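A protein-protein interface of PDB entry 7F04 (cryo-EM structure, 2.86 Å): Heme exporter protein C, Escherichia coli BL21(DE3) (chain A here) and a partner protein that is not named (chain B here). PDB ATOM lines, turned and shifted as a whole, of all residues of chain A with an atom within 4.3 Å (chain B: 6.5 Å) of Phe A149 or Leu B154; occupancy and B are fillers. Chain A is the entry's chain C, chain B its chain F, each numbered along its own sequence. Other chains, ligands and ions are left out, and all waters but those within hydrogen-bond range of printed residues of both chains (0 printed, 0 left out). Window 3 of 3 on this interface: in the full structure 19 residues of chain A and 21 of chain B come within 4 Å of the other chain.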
ATOM      1  N   LEU A 145       7.170 -11.639  -9.231  1.00  0.00           N
ATOM      2  CA  LEU A 145       6.205 -10.954  -8.378  1.00  0.00           C
ATOM      3  C   LEU A 145       5.380 -11.945  -7.571  1.00  0.00           C
ATOM      4  O   LEU A 145       5.102 -11.711  -6.389  1.00  0.00           O
ATOM      5  CB  LEU A 145       5.294 -10.058  -9.214  1.00  0.00           C
ATOM      6  CG  LEU A 145       4.409  -9.119  -8.392  1.00  0.00           C
ATOM      7  CD1 LEU A 145       5.253  -8.136  -7.603  1.00  0.00           C
ATOM      8  CD2 LEU A 145       3.426  -8.389  -9.277  1.00  0.00           C
ATOM      9  N   TRP A 146       4.967 -13.055  -8.188  1.00  0.00           N
ATOM     10  CA  TRP A 146       4.172 -14.033  -7.453  1.00  0.00           C
ATOM     11  C   TRP A 146       4.971 -14.659  -6.317  1.00  0.00           C
ATOM     12  O   TRP A 146       4.433 -14.893  -5.230  1.00  0.00           O
ATOM     13  CB  TRP A 146       3.647 -15.118  -8.391  1.00  0.00           C
ATOM     14  CG  TRP A 146       2.555 -15.926  -7.766  1.00  0.00           C
ATOM     15  CD1 TRP A 146       1.227 -15.623  -7.738  1.00  0.00           C
ATOM     16  CD2 TRP A 146       2.698 -17.162  -7.058  1.00  0.00           C
ATOM     17  NE1 TRP A 146       0.532 -16.595  -7.064  1.00  0.00           N
ATOM     18  CE2 TRP A 146       1.414 -17.551  -6.636  1.00  0.00           C
ATOM     19  CE3 TRP A 146       3.786 -17.979  -6.746  1.00  0.00           C
ATOM     20  CZ2 TRP A 146       1.188 -18.721  -5.921  1.00  0.00           C
ATOM     21  CZ3 TRP A 146       3.560 -19.138  -6.034  1.00  0.00           C
ATOM     22  CH2 TRP A 146       2.272 -19.499  -5.629  1.00  0.00           C
ATOM     23  N   HIS A 147       6.250 -14.937  -6.546  1.00  0.00           N
ATOM     24  CA  HIS A 147       7.083 -15.580  -5.541  1.00  0.00           C
ATOM     25  C   HIS A 147       7.636 -14.613  -4.506  1.00  0.00           C
ATOM     26  O   HIS A 147       8.211 -15.060  -3.512  1.00  0.00           O
ATOM     27  CB  HIS A 147       8.244 -16.318  -6.210  1.00  0.00           C
ATOM     28  CG  HIS A 147       7.855 -17.634  -6.805  1.00  0.00           C
ATOM     29  ND1 HIS A 147       7.864 -17.867  -8.162  1.00  0.00           N
ATOM     30  CD2 HIS A 147       7.439 -18.786  -6.228  1.00  0.00           C
ATOM     31  CE1 HIS A 147       7.473 -19.107  -8.395  1.00  0.00           C
ATOM     32  NE2 HIS A 147       7.209 -19.685  -7.239  1.00  0.00           N
ATOM     33  N   ALA A 148       7.475 -13.309  -4.704  1.00  0.00           N
ATOM     34  CA  ALA A 148       8.031 -12.332  -3.782  1.00  0.00           C
ATOM     35  C   ALA A 148       7.122 -12.042  -2.596  1.00  0.00           C
ATOM     36  O   ALA A 148       7.540 -11.331  -1.678  1.00  0.00           O
ATOM     37  CB  ALA A 148       8.340 -11.028  -4.519  1.00  0.00           C
ATOM     38  N   PHE A 149       5.906 -12.575  -2.586  1.00  0.00           N
ATOM     39  CA  PHE A 149       4.960 -12.350  -1.503  1.00  0.00           C
ATOM     40  C   PHE A 149       4.987 -13.530  -0.543  1.00  0.00           C
ATOM     41  O   PHE A 149       4.816 -14.680  -0.961  1.00  0.00           O
ATOM     42  CB  PHE A 149       3.545 -12.155  -2.043  1.00  0.00           C
ATOM     43  CG  PHE A 149       3.295 -10.797  -2.621  1.00  0.00           C
ATOM     44  CD1 PHE A 149       3.731 -10.483  -3.894  1.00  0.00           C
ATOM     45  CD2 PHE A 149       2.615  -9.836  -1.897  1.00  0.00           C
ATOM     46  CE1 PHE A 149       3.500  -9.236  -4.431  1.00  0.00           C
ATOM     47  CE2 PHE A 149       2.381  -8.586  -2.429  1.00  0.00           C
ATOM     48  CZ  PHE A 149       2.825  -8.287  -3.697  1.00  0.00           C
ATOM     49  N   ASP A 150       5.204 -13.242   0.741  1.00  0.00           N
ATOM     50  CA  ASP A 150       5.126 -14.291   1.751  1.00  0.00           C
ATOM     51  C   ASP A 150       3.709 -14.838   1.865  1.00  0.00           C
ATOM     52  O   ASP A 150       3.514 -16.051   2.002  1.00  0.00           O
ATOM     53  CB  ASP A 150       5.606 -13.760   3.101  1.00  0.00           C
ATOM     54  CG  ASP A 150       7.115 -13.732   3.214  1.00  0.00           C
ATOM     55  OD1 ASP A 150       7.722 -14.813   3.361  1.00  0.00           O
ATOM     56  OD2 ASP A 150       7.697 -12.628   3.160  1.00  0.00           O
ATOM     57  N   ASP A 151       2.711 -13.961   1.805  1.00  0.00           N
ATOM     58  CA  ASP A 151       1.319 -14.351   1.973  1.00  0.00           C
ATOM     59  C   ASP A 151       0.692 -14.625   0.612  1.00  0.00           C
ATOM     60  O   ASP A 151       0.661 -13.744  -0.251  1.00  0.00           O
ATOM     61  CB  ASP A 151       0.541 -13.261   2.707  1.00  0.00           C
ATOM     62  CG  ASP A 151      -0.881 -13.674   3.028  1.00  0.00           C
ATOM     63  OD1 ASP A 151      -1.069 -14.521   3.927  1.00  0.00           O
ATOM     64  OD2 ASP A 151      -1.813 -13.146   2.386  1.00  0.00           O
ATOM     65  N   ARG A 152       0.191 -15.843   0.429  1.00  0.00           N
ATOM     66  CA  ARG A 152      -0.561 -16.168  -0.769  1.00  0.00           C
ATOM     67  C   ARG A 152      -1.935 -15.502  -0.715  1.00  0.00           C
ATOM     68  O   ARG A 152      -2.336 -14.921   0.297  1.00  0.00           O
ATOM     69  CB  ARG A 152      -0.702 -17.681  -0.923  1.00  0.00           C
ATOM     70  CG  ARG A 152       0.594 -18.402  -1.256  1.00  0.00           C
ATOM     71  CD  ARG A 152       1.345 -17.711  -2.378  1.00  0.00           C
ATOM     72  NE  ARG A 152       2.772 -18.006  -2.341  1.00  0.00           N
ATOM     73  CZ  ARG A 152       3.727 -17.119  -2.587  1.00  0.00           C
ATOM     74  NH1 ARG A 152       3.443 -15.864  -2.888  1.00  0.00           N
ATOM     75  NH2 ARG A 152       4.999 -17.503  -2.533  1.00  0.00           N
ATOM     76  N   ALA A 155      -0.406 -12.594  -3.508  1.00  0.00           N
ATOM     77  CA  ALA A 155       0.275 -12.883  -4.762  1.00  0.00           C
ATOM     78  C   ALA A 155      -0.699 -13.662  -5.633  1.00  0.00           C
ATOM     79  O   ALA A 155      -1.088 -14.783  -5.293  1.00  0.00           O
ATOM     80  CB  ALA A 155       1.553 -13.673  -4.517  1.00  0.00           C
ATOM     81  N   ALA A 158      -1.739  -9.297  -6.982  1.00  0.00           N
ATOM     82  CA  ALA A 158      -0.633  -8.529  -7.536  1.00  0.00           C
ATOM     83  C   ALA A 158      -0.165  -9.117  -8.859  1.00  0.00           C
ATOM     84  O   ALA A 158       0.100  -8.381  -9.817  1.00  0.00           O
ATOM     85  CB  ALA A 158       0.520  -8.475  -6.535  1.00  0.00           C
ATOM     86  N   LEU B  74       4.305   3.124   3.450  1.00  0.00           N
ATOM     87  CA  LEU B  74       3.758   1.913   4.043  1.00  0.00           C
ATOM     88  C   LEU B  74       4.182   1.761   5.498  1.00  0.00           C
ATOM     89  O   LEU B  74       3.406   1.256   6.316  1.00  0.00           O
ATOM     90  CB  LEU B  74       4.184   0.692   3.233  1.00  0.00           C
ATOM     91  CG  LEU B  74       3.579  -0.630   3.700  1.00  0.00           C
ATOM     92  CD1 LEU B  74       2.066  -0.612   3.539  1.00  0.00           C
ATOM     93  CD2 LEU B  74       4.189  -1.791   2.951  1.00  0.00           C
ATOM     94  N   LEU B 150       2.958  -2.217  -6.591  1.00  0.00           N
ATOM     95  CA  LEU B 150       2.888  -3.657  -6.372  1.00  0.00           C
ATOM     96  C   LEU B 150       4.000  -4.133  -5.446  1.00  0.00           C
ATOM     97  O   LEU B 150       3.791  -5.040  -4.633  1.00  0.00           O
ATOM     98  CB  LEU B 150       2.957  -4.396  -7.707  1.00  0.00           C
ATOM     99  CG  LEU B 150       1.746  -4.297  -8.633  1.00  0.00           C
ATOM    100  CD1 LEU B 150       2.115  -4.736 -10.037  1.00  0.00           C
ATOM    101  CD2 LEU B 150       0.596  -5.125  -8.100  1.00  0.00           C
ATOM    102  N   THR B 151       5.186  -3.539  -5.553  1.00  0.00           N
ATOM    103  CA  THR B 151       6.347  -3.989  -4.800  1.00  0.00           C
ATOM    104  C   THR B 151       6.578  -3.203  -3.514  1.00  0.00           C
ATOM    105  O   THR B 151       7.599  -3.413  -2.853  1.00  0.00           O
ATOM    106  CB  THR B 151       7.602  -3.922  -5.675  1.00  0.00           C
ATOM    107  OG1 THR B 151       7.821  -2.570  -6.094  1.00  0.00           O
ATOM    108  CG2 THR B 151       7.444  -4.803  -6.899  1.00  0.00           C
ATOM    109  N   VAL B 152       5.666  -2.301  -3.145  1.00  0.00           N
ATOM    110  CA  VAL B 152       5.881  -1.487  -1.952  1.00  0.00           C
ATOM    111  C   VAL B 152       5.831  -2.346  -0.693  1.00  0.00           C
ATOM    112  O   VAL B 152       6.576  -2.108   0.265  1.00  0.00           O
ATOM    113  CB  VAL B 152       4.869  -0.326  -1.898  1.00  0.00           C
ATOM    114  CG1 VAL B 152       3.445  -0.838  -1.755  1.00  0.00           C
ATOM    115  CG2 VAL B 152       5.212   0.623  -0.766  1.00  0.00           C
ATOM    116  N   GLY B 153       4.962  -3.359  -0.673  1.00  0.00           N
ATOM    117  CA  GLY B 153       4.883  -4.235   0.491  1.00  0.00           C
ATOM    118  C   GLY B 153       6.142  -5.073   0.647  1.00  0.00           C
ATOM    119  O   GLY B 153       6.531  -5.406   1.772  1.00  0.00           O
ATOM    120  N   LEU B 154       6.786  -5.420  -0.465  1.00  0.00           N
ATOM    121  CA  LEU B 154       7.982  -6.251  -0.414  1.00  0.00           C
ATOM    122  C   LEU B 154       9.198  -5.457   0.040  1.00  0.00           C
ATOM    123  O   LEU B 154      10.072  -6.003   0.723  1.00  0.00           O
ATOM    124  CB  LEU B 154       8.224  -6.871  -1.786  1.00  0.00           C
ATOM    125  CG  LEU B 154       6.921  -7.289  -2.471  1.00  0.00           C
ATOM    126  CD1 LEU B 154       7.174  -7.740  -3.892  1.00  0.00           C
ATOM    127  CD2 LEU B 154       6.220  -8.375  -1.676  1.00  0.00           C
ATOM    128  N   LYS B 155       9.263  -4.176  -0.321  1.00  0.00           N
ATOM    129  CA  LYS B 155      10.377  -3.291   0.016  1.00  0.00           C
ATOM    130  C   LYS B 155      11.712  -3.938  -0.357  1.00  0.00           C
ATOM    131  O   LYS B 155      12.660  -3.996   0.428  1.00  0.00           O
ATOM    132  CB  LYS B 155      10.339  -2.896   1.495  1.00  0.00           C
ATOM    133  CG  LYS B 155      11.175  -1.672   1.841  1.00  0.00           C
ATOM    134  CD  LYS B 155      11.193  -1.424   3.338  1.00  0.00           C
ATOM    135  CE  LYS B 155      12.092  -2.424   4.046  1.00  0.00           C
ATOM    136  NZ  LYS B 155      12.294  -2.075   5.479  1.00  0.00           N
ATOM    137  N   ARG B 156      11.755  -4.451  -1.584  1.00  0.00           N
ATOM    138  CA  ARG B 156      12.972  -5.041  -2.128  1.00  0.00           C
ATOM    139  C   ARG B 156      14.079  -3.997  -2.232  1.00  0.00           C
ATOM    140  O   ARG B 156      15.215  -4.242  -1.814  1.00  0.00           O
ATOM    141  CB  ARG B 156      12.681  -5.660  -3.499  1.00  0.00           C
ATOM    142  CG  ARG B 156      11.722  -6.831  -3.444  1.00  0.00           C
ATOM    143  CD  ARG B 156      12.391  -8.058  -2.865  1.00  0.00           C
ATOM    144  NE  ARG B 156      11.469  -9.183  -2.773  1.00  0.00           N
ATOM    145  CZ  ARG B 156      11.794 -10.375  -2.295  1.00  0.00           C
ATOM    146  NH1 ARG B 156      13.027 -10.649  -1.903  1.00  0.00           N
ATOM    147  NH2 ARG B 156      10.862 -11.318  -2.215  1.00  0.00           N
ATOM    148  N   GLY B 157      13.753  -2.824  -2.766  1.00  0.00           N
ATOM    149  CA  GLY B 157      14.768  -1.811  -2.999  1.00  0.00           C
ATOM    150  C   GLY B 157      15.884  -2.309  -3.887  1.00  0.00           C
ATOM    151  O   GLY B 157      17.057  -2.013  -3.632  1.00  0.00           O
ATOM    152  N   LEU B 160      14.048  -6.263  -8.349  1.00  0.00           N
ATOM    153  CA  LEU B 160      12.690  -6.700  -8.657  1.00  0.00           C
ATOM    154  C   LEU B 160      11.902  -5.611  -9.368  1.00  0.00           C
ATOM    155  O   LEU B 160      11.222  -5.879 -10.363  1.00  0.00           O
ATOM    156  CB  LEU B 160      11.966  -7.134  -7.384  1.00  0.00           C
ATOM    157  CG  LEU B 160      10.545  -7.651  -7.622  1.00  0.00           C
ATOM    158  CD1 LEU B 160      10.557  -8.777  -8.635  1.00  0.00           C
ATOM    159  CD2 LEU B 160       9.905  -8.108  -6.329  1.00  0.00           C
ATOM    160  N   ILE B 217      -4.329  -3.615  -3.088  1.00  0.00           N
ATOM    161  CA  ILE B 217      -3.853  -4.986  -2.910  1.00  0.00           C
ATOM    162  C   ILE B 217      -2.766  -5.036  -1.844  1.00  0.00           C
ATOM    163  O   ILE B 217      -2.773  -5.906  -0.966  1.00  0.00           O
ATOM    164  CB  ILE B 217      -3.348  -5.564  -4.246  1.00  0.00           C
ATOM    165  CG1 ILE B 217      -4.451  -5.579  -5.308  1.00  0.00           C
ATOM    166  CG2 ILE B 217      -2.781  -6.956  -4.044  1.00  0.00           C
ATOM    167  CD1 ILE B 217      -5.813  -5.970  -4.799  1.00  0.00           C
ATOM    168  N   SER B 218      -1.817  -4.099  -1.901  1.00  0.00           N
ATOM    169  CA  SER B 218      -0.648  -4.163  -1.030  1.00  0.00           C
ATOM    170  C   SER B 218      -0.973  -3.776   0.406  1.00  0.00           C
ATOM    171  O   SER B 218      -0.329  -4.273   1.336  1.00  0.00           O
ATOM    172  CB  SER B 218       0.461  -3.265  -1.575  1.00  0.00           C
ATOM    173  OG  SER B 218       0.765  -3.591  -2.919  1.00  0.00           O
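The backbone carbonyl oxygen (O) of Phe A149 is in hydrogen-bond range of the guanidinium group (NH1) of Arg A152 (2.6 Å).
The backbone carbonyl oxygen (O) of Ala A148 sits at hydrogen-bond distance from the guanidinium group (NH2) of Arg B156, at 3.4 Å.
CD1 of Leu B150 touches CD2 of Leu A145, 3.95 Å away. CD2 of Leu B154 touches O of Ala A148 (3.2 Å). Ala A148 touches Leu B160 (CB to CD2, 3.8 Å). Phe A149 touches Leu B150 (CZ to O, 3.5 Å). Phe A149 touches Leu B154 (CD2 to CD2, 3.9 Å). Ala A158 touches Leu B150. Ala A158 touches Ile B217 (N to CG2, 3.9 Å).
Of the 12 printed residues of chain B, 5 touch a printed residue of chain A. Printed residues of chain B that touch a printed residue of chain A: Leu B150, Leu B154, Arg B156, Leu B160 and Ile B217. Hydrophobic or aromatic side chains of chain A that line the printed part of chain B: Leu A145, Ala A148, Phe A149 and Ala A158. Among the printed residues, no Asp or Glu carboxylate lies within 4 Å of a Lys or Arg side-chain nitrogen of the other chain.
Of chain B, only Leu B150 (3.5 Å) and Leu B154 (3.9 Å) come within 4 Å of Phe A149. Leu B154 touches two residues of chain A. Printed residues of chain B within 4 Å of Ala A148: Leu B154 (3.2 Å), Arg B156 (3.4 Å) and Leu B160 (3.8 Å). Of the printed residues of chain A, Leu B160 touches Ala A148 (3.8 Å). Printed residues of chain A within 4 Å of Leu B150: Leu A145, Phe A149 and Ala A158. Of the printed residues of chain A, Ile B217 touches Ala A158. Printed residues of chain B within 4 Å of Leu A145: Leu B150 (3.95 Å). Trp A146 touches none of the printed residues of chain B. The nearest residue of chain B that does not touch Phe A149 is Arg B156 (5.1 Å). The nearest printed residue of chain B that does not touch Leu A145 is Thr B151 (4.1 Å).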
